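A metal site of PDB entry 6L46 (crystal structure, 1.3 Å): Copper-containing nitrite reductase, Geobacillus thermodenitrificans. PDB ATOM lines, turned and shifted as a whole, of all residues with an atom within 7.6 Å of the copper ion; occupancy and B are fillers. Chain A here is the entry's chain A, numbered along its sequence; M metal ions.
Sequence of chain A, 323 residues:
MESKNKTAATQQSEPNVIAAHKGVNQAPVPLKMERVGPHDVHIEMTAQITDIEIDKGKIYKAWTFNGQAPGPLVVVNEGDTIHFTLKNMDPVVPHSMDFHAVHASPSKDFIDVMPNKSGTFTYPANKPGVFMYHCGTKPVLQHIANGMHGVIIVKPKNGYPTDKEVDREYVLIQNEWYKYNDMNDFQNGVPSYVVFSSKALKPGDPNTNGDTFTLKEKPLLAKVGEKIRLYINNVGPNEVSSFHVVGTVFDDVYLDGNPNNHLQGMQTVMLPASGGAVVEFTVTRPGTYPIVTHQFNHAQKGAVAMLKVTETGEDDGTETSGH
The side-chain sulfur (SG) of Cys 135 sits close to the backbone NH (N) of Ser 96, 3.5 Å away.
The backbone carbonyl oxygen (O) of Trp 63 lies close to the backbone NH (N) of Met 148 (3.2 Å).
NE2 of His 95 lies within hydrogen-bond range of OD2 of Asp 90 (2.7 Å).
A ring nitrogen (NE2) of His 95 lies close to the backbone carbonyl oxygen (O) of Val 93 (3.4 Å).
The side-chain sulfur of Cys 135 lies close to the side-chain hydroxyl of Thr 137 (3.4 Å).
ND2 of Asn 88 sits close to N of His 95 (3.5 Å).
Within 4 Å of the copper ion: His 95, Cys 135, His 143 and Met 148.
The copper ion is bound by ND1 of His 143 (1.9 Å), ND1 of His 95 (2.0 Å), SG of Cys 135 (2.2 Å) and SD of Met 148 (2.6 Å).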
ATOM      1  N   ALA A  47      16.279  -2.565 -34.597  1.00  0.00           N
ATOM      2  CA  ALA A  47      16.207  -2.530 -33.152  1.00  0.00           C
ATOM      3  C   ALA A  47      16.606  -1.111 -32.778  1.00  0.00           C
ATOM      4  O   ALA A  47      17.630  -0.610 -33.242  1.00  0.00           O
ATOM      5  CB  ALA A  47      17.203  -3.505 -32.510  1.00  0.00           C
ATOM      6  N   TRP A  63      13.033  -0.494 -25.493  1.00  0.00           N
ATOM      7  CA  TRP A  63      13.810  -1.229 -26.467  1.00  0.00           C
ATOM      8  C   TRP A  63      12.811  -1.803 -27.446  1.00  0.00           C
ATOM      9  O   TRP A  63      11.876  -2.495 -27.037  1.00  0.00           O
ATOM     10  CB  TRP A  63      14.556  -2.377 -25.794  1.00  0.00           C
ATOM     11  CG  TRP A  63      15.517  -1.980 -24.738  1.00  0.00           C
ATOM     12  CD1 TRP A  63      15.723  -0.746 -24.176  1.00  0.00           C
ATOM     13  CD2 TRP A  63      16.439  -2.862 -24.112  1.00  0.00           C
ATOM     14  NE1 TRP A  63      16.723  -0.831 -23.240  1.00  0.00           N
ATOM     15  CE2 TRP A  63      17.170  -2.119 -23.178  1.00  0.00           C
ATOM     16  CE3 TRP A  63      16.687  -4.226 -24.252  1.00  0.00           C
ATOM     17  CZ2 TRP A  63      18.159  -2.707 -22.375  1.00  0.00           C
ATOM     18  CZ3 TRP A  63      17.656  -4.809 -23.440  1.00  0.00           C
ATOM     19  CH2 TRP A  63      18.380  -4.055 -22.525  1.00  0.00           C
ATOM     20  N   THR A  64      12.986  -1.482 -28.726  1.00  0.00           N
ATOM     21  CA  THR A  64      11.916  -1.750 -29.665  1.00  0.00           C
ATOM     22  C   THR A  64      12.437  -2.319 -30.955  1.00  0.00           C
ATOM     23  O   THR A  64      13.614  -2.175 -31.313  1.00  0.00           O
ATOM     24  CB  THR A  64      11.131  -0.493 -30.050  1.00  0.00           C
ATOM     25  OG1 THR A  64      11.921   0.327 -30.921  1.00  0.00           O
ATOM     26  CG2 THR A  64      10.723   0.323 -28.838  1.00  0.00           C
ATOM     27  N   PHE A  65      11.513  -2.916 -31.693  1.00  0.00           N
ATOM     28  CA  PHE A  65      11.656  -3.052 -33.115  1.00  0.00           C
ATOM     29  C   PHE A  65      10.957  -1.867 -33.774  1.00  0.00           C
ATOM     30  O   PHE A  65       9.766  -1.638 -33.532  1.00  0.00           O
ATOM     31  CB  PHE A  65      11.034  -4.353 -33.590  1.00  0.00           C
ATOM     32  CG  PHE A  65      11.726  -5.565 -33.045  1.00  0.00           C
ATOM     33  CD1 PHE A  65      12.968  -5.951 -33.544  1.00  0.00           C
ATOM     34  CD2 PHE A  65      11.142  -6.305 -32.022  1.00  0.00           C
ATOM     35  CE1 PHE A  65      13.605  -7.073 -33.024  1.00  0.00           C
ATOM     36  CE2 PHE A  65      11.775  -7.448 -31.525  1.00  0.00           C
ATOM     37  CZ  PHE A  65      13.007  -7.829 -32.036  1.00  0.00           C
ATOM     38  N   LEU A  86      17.795  -7.552 -39.562  1.00  0.00           N
ATOM     39  CA  LEU A  86      17.707  -6.679 -38.401  1.00  0.00           C
ATOM     40  C   LEU A  86      18.854  -5.699 -38.474  1.00  0.00           C
ATOM     41  O   LEU A  86      20.016  -6.095 -38.526  1.00  0.00           O
ATOM     42  CB  LEU A  86      17.814  -7.473 -37.112  1.00  0.00           C
ATOM     43  CG  LEU A  86      17.647  -6.637 -35.848  1.00  0.00           C
ATOM     44  CD1 LEU A  86      16.253  -6.029 -35.756  1.00  0.00           C
ATOM     45  CD2 LEU A  86      17.912  -7.524 -34.635  1.00  0.00           C
ATOM     46  N   ASN A  88      20.542  -3.063 -36.242  1.00  0.00           N
ATOM     47  CA  ASN A  88      20.577  -2.704 -34.834  1.00  0.00           C
ATOM     48  C   ASN A  88      21.050  -1.267 -34.700  1.00  0.00           C
ATOM     49  O   ASN A  88      22.222  -0.966 -34.898  1.00  0.00           O
ATOM     50  CB  ASN A  88      21.479  -3.650 -34.048  1.00  0.00           C
ATOM     51  CG  ASN A  88      21.396  -3.403 -32.581  1.00  0.00           C
ATOM     52  OD1 ASN A  88      20.623  -2.554 -32.133  1.00  0.00           O
ATOM     53  ND2 ASN A  88      22.173  -4.127 -31.797  1.00  0.00           N
ATOM     54  N   ASP A  90      20.624   0.346 -31.777  1.00  0.00           N
ATOM     55  CA  ASP A  90      20.966   0.579 -30.397  1.00  0.00           C
ATOM     56  C   ASP A  90      22.462   0.839 -30.333  1.00  0.00           C
ATOM     57  O   ASP A  90      23.240   0.080 -30.896  1.00  0.00           O
ATOM     58  CB  ASP A  90      20.620  -0.693 -29.627  1.00  0.00           C
ATOM     59  CG  ASP A  90      20.759  -0.554 -28.122  1.00  0.00           C
ATOM     60  OD1 ASP A  90      21.743   0.062 -27.658  1.00  0.00           O
ATOM     61  OD2 ASP A  90      19.906  -1.111 -27.406  1.00  0.00           O
ATOM     62  N   VAL A  93      23.637  -2.084 -26.991  1.00  0.00           N
ATOM     63  CA  VAL A  93      23.105  -3.403 -26.650  1.00  0.00           C
ATOM     64  C   VAL A  93      22.895  -4.202 -27.930  1.00  0.00           C
ATOM     65  O   VAL A  93      22.245  -3.709 -28.846  1.00  0.00           O
ATOM     66  CB  VAL A  93      21.789  -3.322 -25.853  1.00  0.00           C
ATOM     67  CG1 VAL A  93      21.418  -4.715 -25.367  1.00  0.00           C
ATOM     68  CG2 VAL A  93      21.913  -2.370 -24.684  1.00  0.00           C
ATOM     69  N   PRO A  94      23.396  -5.430 -28.003  1.00  0.00           N
ATOM     70  CA  PRO A  94      23.026  -6.294 -29.125  1.00  0.00           C
ATOM     71  C   PRO A  94      21.560  -6.648 -29.062  1.00  0.00           C
ATOM     72  O   PRO A  94      20.954  -6.667 -27.989  1.00  0.00           O
ATOM     73  CB  PRO A  94      23.874  -7.553 -28.888  1.00  0.00           C
ATOM     74  CG  PRO A  94      24.990  -7.098 -27.997  1.00  0.00           C
ATOM     75  CD  PRO A  94      24.325  -6.083 -27.086  1.00  0.00           C
ATOM     76  N   HIS A  95      20.999  -6.977 -30.225  1.00  0.00           N
ATOM     77  CA  HIS A  95      19.639  -7.441 -30.293  1.00  0.00           C
ATOM     78  C   HIS A  95      19.534  -8.522 -31.344  1.00  0.00           C
ATOM     79  O   HIS A  95      20.453  -8.744 -32.132  1.00  0.00           O
ATOM     80  CB  HIS A  95      18.664  -6.303 -30.598  1.00  0.00           C
ATOM     81  CG  HIS A  95      18.652  -5.260 -29.547  1.00  0.00           C
ATOM     82  ND1 HIS A  95      18.080  -5.458 -28.296  1.00  0.00           N
ATOM     83  CD2 HIS A  95      19.172  -4.013 -29.543  1.00  0.00           C
ATOM     84  CE1 HIS A  95      18.277  -4.369 -27.572  1.00  0.00           C
ATOM     85  NE2 HIS A  95      18.928  -3.477 -28.306  1.00  0.00           N
ATOM     86  N   SER A  96      18.394  -9.201 -31.344  1.00  0.00           N
ATOM     87  CA  SER A  96      18.200 -10.330 -32.221  1.00  0.00           C
ATOM     88  C   SER A  96      16.712 -10.459 -32.476  1.00  0.00           C
ATOM     89  O   SER A  96      15.912  -9.720 -31.898  1.00  0.00           O
ATOM     90  CB  SER A  96      18.712 -11.610 -31.573  1.00  0.00           C
ATOM     91  OG  SER A  96      18.048 -11.819 -30.344  1.00  0.00           O
ATOM     92  N   MET A  97      16.352 -11.424 -33.313  1.00  0.00           N
ATOM     93  CA  MET A  97      14.958 -11.658 -33.626  1.00  0.00           C
ATOM     94  C   MET A  97      14.672 -13.151 -33.587  1.00  0.00           C
ATOM     95  O   MET A  97      15.374 -13.946 -34.217  1.00  0.00           O
ATOM     96  CB  MET A  97      14.613 -11.124 -35.019  1.00  0.00           C
ATOM     97  CG  MET A  97      13.220 -11.520 -35.499  1.00  0.00           C
ATOM     98  SD  MET A  97      11.908 -10.854 -34.450  1.00  0.00           S
ATOM     99  CE  MET A  97      11.755  -9.227 -35.189  1.00  0.00           C
ATOM    100  N   ASP A 112      22.664 -12.721 -32.217  1.00  0.00           N
ATOM    101  CA  ASP A 112      22.765 -11.304 -31.960  1.00  0.00           C
ATOM    102  C   ASP A 112      23.360 -10.552 -33.140  1.00  0.00           C
ATOM    103  O   ASP A 112      24.241 -11.032 -33.842  1.00  0.00           O
ATOM    104  CB  ASP A 112      23.602 -11.058 -30.712  1.00  0.00           C
ATOM    105  CG  ASP A 112      22.913 -11.532 -29.456  1.00  0.00           C
ATOM    106  OD1 ASP A 112      21.671 -11.689 -29.470  1.00  0.00           O
ATOM    107  OD2 ASP A 112      23.597 -11.752 -28.440  1.00  0.00           O
ATOM    108  N   HIS A 134       9.964 -11.853 -30.949  1.00  0.00           N
ATOM    109  CA  HIS A 134      10.579 -11.077 -29.889  1.00  0.00           C
ATOM    110  C   HIS A 134      12.078 -11.120 -30.051  1.00  0.00           C
ATOM    111  O   HIS A 134      12.622 -11.994 -30.723  1.00  0.00           O
ATOM    112  CB  HIS A 134      10.153 -11.603 -28.523  1.00  0.00           C
ATOM    113  CG  HIS A 134      10.499 -13.041 -28.270  1.00  0.00           C
ATOM    114  ND1 HIS A 134      11.729 -13.445 -27.823  1.00  0.00           N
ATOM    115  CD2 HIS A 134       9.753 -14.175 -28.383  1.00  0.00           C
ATOM    116  CE1 HIS A 134      11.738 -14.762 -27.662  1.00  0.00           C
ATOM    117  NE2 HIS A 134      10.542 -15.229 -27.992  1.00  0.00           N
ATOM    118  N   CYS A 135      12.744 -10.194 -29.391  1.00  0.00           N
ATOM    119  CA  CYS A 135      14.186 -10.266 -29.302  1.00  0.00           C
ATOM    120  C   CYS A 135      14.583 -11.496 -28.499  1.00  0.00           C
ATOM    121  O   CYS A 135      13.947 -11.825 -27.501  1.00  0.00           O
ATOM    122  CB  CYS A 135      14.692  -8.998 -28.648  1.00  0.00           C
ATOM    123  SG  CYS A 135      16.461  -8.969 -28.480  1.00  0.00           S
ATOM    124  N   GLY A 136      15.646 -12.156 -28.930  1.00  0.00           N
ATOM    125  CA  GLY A 136      16.117 -13.377 -28.332  1.00  0.00           C
ATOM    126  C   GLY A 136      17.472 -13.258 -27.683  1.00  0.00           C
ATOM    127  O   GLY A 136      18.144 -14.255 -27.478  1.00  0.00           O
ATOM    128  N   THR A 137      17.885 -12.044 -27.338  1.00  0.00           N
ATOM    129  CA  THR A 137      19.194 -11.789 -26.768  1.00  0.00           C
ATOM    130  C   THR A 137      19.136 -11.960 -25.267  1.00  0.00           C
ATOM    131  O   THR A 137      18.200 -11.504 -24.612  1.00  0.00           O
ATOM    132  CB  THR A 137      19.596 -10.367 -27.141  1.00  0.00           C
ATOM    133  OG1 THR A 137      19.642 -10.272 -28.561  1.00  0.00           O
ATOM    134  CG2 THR A 137      20.951  -9.984 -26.531  1.00  0.00           C
ATOM    135  N   LYS A 138      20.124 -12.634 -24.718  1.00  0.00           N
ATOM    136  CA  LYS A 138      20.118 -12.860 -23.289  1.00  0.00           C
ATOM    137  C   LYS A 138      20.461 -11.570 -22.543  1.00  0.00           C
ATOM    138  O   LYS A 138      21.335 -10.815 -22.992  1.00  0.00           O
ATOM    139  CB  LYS A 138      21.139 -13.937 -22.905  1.00  0.00           C
ATOM    140  CG  LYS A 138      20.750 -15.319 -23.384  1.00  0.00           C
ATOM    141  CD  LYS A 138      21.760 -16.364 -22.961  1.00  0.00           C
ATOM    142  CE  LYS A 138      21.676 -16.693 -21.476  1.00  0.00           C
ATOM    143  NZ  LYS A 138      22.744 -17.626 -21.022  1.00  0.00           N
ATOM    144  N   PRO A 139      19.798 -11.284 -21.423  1.00  0.00           N
ATOM    145  CA  PRO A 139      18.688 -12.048 -20.856  1.00  0.00           C
ATOM    146  C   PRO A 139      17.416 -11.761 -21.648  1.00  0.00           C
ATOM    147  O   PRO A 139      17.013 -10.596 -21.808  1.00  0.00           O
ATOM    148  CB  PRO A 139      18.537 -11.471 -19.440  1.00  0.00           C
ATOM    149  CG  PRO A 139      19.757 -10.647 -19.209  1.00  0.00           C
ATOM    150  CD  PRO A 139      20.180 -10.168 -20.563  1.00  0.00           C
ATOM    151  N   VAL A 140      16.769 -12.808 -22.141  1.00  0.00           N
ATOM    152  CA  VAL A 140      15.610 -12.613 -22.998  1.00  0.00           C
ATOM    153  C   VAL A 140      14.518 -11.867 -22.254  1.00  0.00           C
ATOM    154  O   VAL A 140      13.850 -11.006 -22.817  1.00  0.00           O
ATOM    155  CB  VAL A 140      15.135 -13.967 -23.547  1.00  0.00           C
ATOM    156  CG1 VAL A 140      13.839 -13.782 -24.330  1.00  0.00           C
ATOM    157  CG2 VAL A 140      16.234 -14.534 -24.436  1.00  0.00           C
ATOM    158  N   GLN A 142      14.815  -9.527 -20.203  1.00  0.00           N
ATOM    159  CA  GLN A 142      15.095  -8.104 -20.239  1.00  0.00           C
ATOM    160  C   GLN A 142      14.716  -7.501 -21.582  1.00  0.00           C
ATOM    161  O   GLN A 142      14.154  -6.407 -21.648  1.00  0.00           O
ATOM    162  CB  GLN A 142      16.585  -7.877 -19.963  1.00  0.00           C
ATOM    163  CG  GLN A 142      16.958  -6.430 -19.834  1.00  0.00           C
ATOM    164  CD  GLN A 142      18.380  -6.248 -19.428  1.00  0.00           C
ATOM    165  OE1 GLN A 142      19.190  -7.165 -19.535  1.00  0.00           O
ATOM    166  NE2 GLN A 142      18.693  -5.076 -18.936  1.00  0.00           N
ATOM    167  N   HIS A 143      15.078  -8.184 -22.660  1.00  0.00           N
ATOM    168  CA  HIS A 143      14.789  -7.652 -23.974  1.00  0.00           C
ATOM    169  C   HIS A 143      13.296  -7.630 -24.246  1.00  0.00           C
ATOM    170  O   HIS A 143      12.778  -6.653 -24.807  1.00  0.00           O
ATOM    171  CB  HIS A 143      15.556  -8.430 -25.020  1.00  0.00           C
ATOM    172  CG  HIS A 143      17.004  -8.125 -24.992  1.00  0.00           C
ATOM    173  ND1 HIS A 143      17.617  -7.346 -25.966  1.00  0.00           N
ATOM    174  CD2 HIS A 143      17.970  -8.436 -24.098  1.00  0.00           C
ATOM    175  CE1 HIS A 143      18.899  -7.218 -25.672  1.00  0.00           C
ATOM    176  NE2 HIS A 143      19.139  -7.874 -24.541  1.00  0.00           N
ATOM    177  N   ILE A 144      12.578  -8.682 -23.851  1.00  0.00           N
ATOM    178  CA  ILE A 144      11.137  -8.668 -24.036  1.00  0.00           C
ATOM    179  C   ILE A 144      10.497  -7.601 -23.166  1.00  0.00           C
ATOM    180  O   ILE A 144       9.692  -6.792 -23.636  1.00  0.00           O
ATOM    181  CB  ILE A 144      10.528 -10.047 -23.743  1.00  0.00           C
ATOM    182  CG1 ILE A 144      11.072 -11.096 -24.726  1.00  0.00           C
ATOM    183  CG2 ILE A 144       8.999  -9.940 -23.851  1.00  0.00           C
ATOM    184  CD1 ILE A 144      10.539 -12.503 -24.441  1.00  0.00           C
ATOM    185  N   ASN A 146      11.524  -4.933 -21.901  1.00  0.00           N
ATOM    186  CA  ASN A 146      11.787  -3.559 -22.322  1.00  0.00           C
ATOM    187  C   ASN A 146      11.084  -3.176 -23.611  1.00  0.00           C
ATOM    188  O   ASN A 146      11.137  -1.991 -23.970  1.00  0.00           O
ATOM    189  CB  ASN A 146      13.276  -3.292 -22.442  1.00  0.00           C
ATOM    190  CG  ASN A 146      13.926  -3.044 -21.100  1.00  0.00           C
ATOM    191  OD1 ASN A 146      13.321  -2.459 -20.193  1.00  0.00           O
ATOM    192  ND2 ASN A 146      15.158  -3.476 -20.982  1.00  0.00           N
ATOM    193  N   MET A 148      10.693  -5.501 -26.698  1.00  0.00           N
ATOM    194  CA  MET A 148      11.045  -6.142 -27.971  1.00  0.00           C
ATOM    195  C   MET A 148      10.198  -7.387 -28.176  1.00  0.00           C
ATOM    196  O   MET A 148      10.669  -8.527 -28.063  1.00  0.00           O
ATOM    197  CB  MET A 148      12.528  -6.449 -28.029  1.00  0.00           C
ATOM    198  CG  MET A 148      13.343  -5.220 -27.724  1.00  0.00           C
ATOM    199  SD  MET A 148      15.059  -5.304 -28.206  1.00  0.00           S
ATOM    200  CE  MET A 148      14.944  -5.231 -29.977  1.00  0.00           C
HETATM  201 CU    CU M   1      16.959  -6.981 -27.757  1.00  0.00          CU
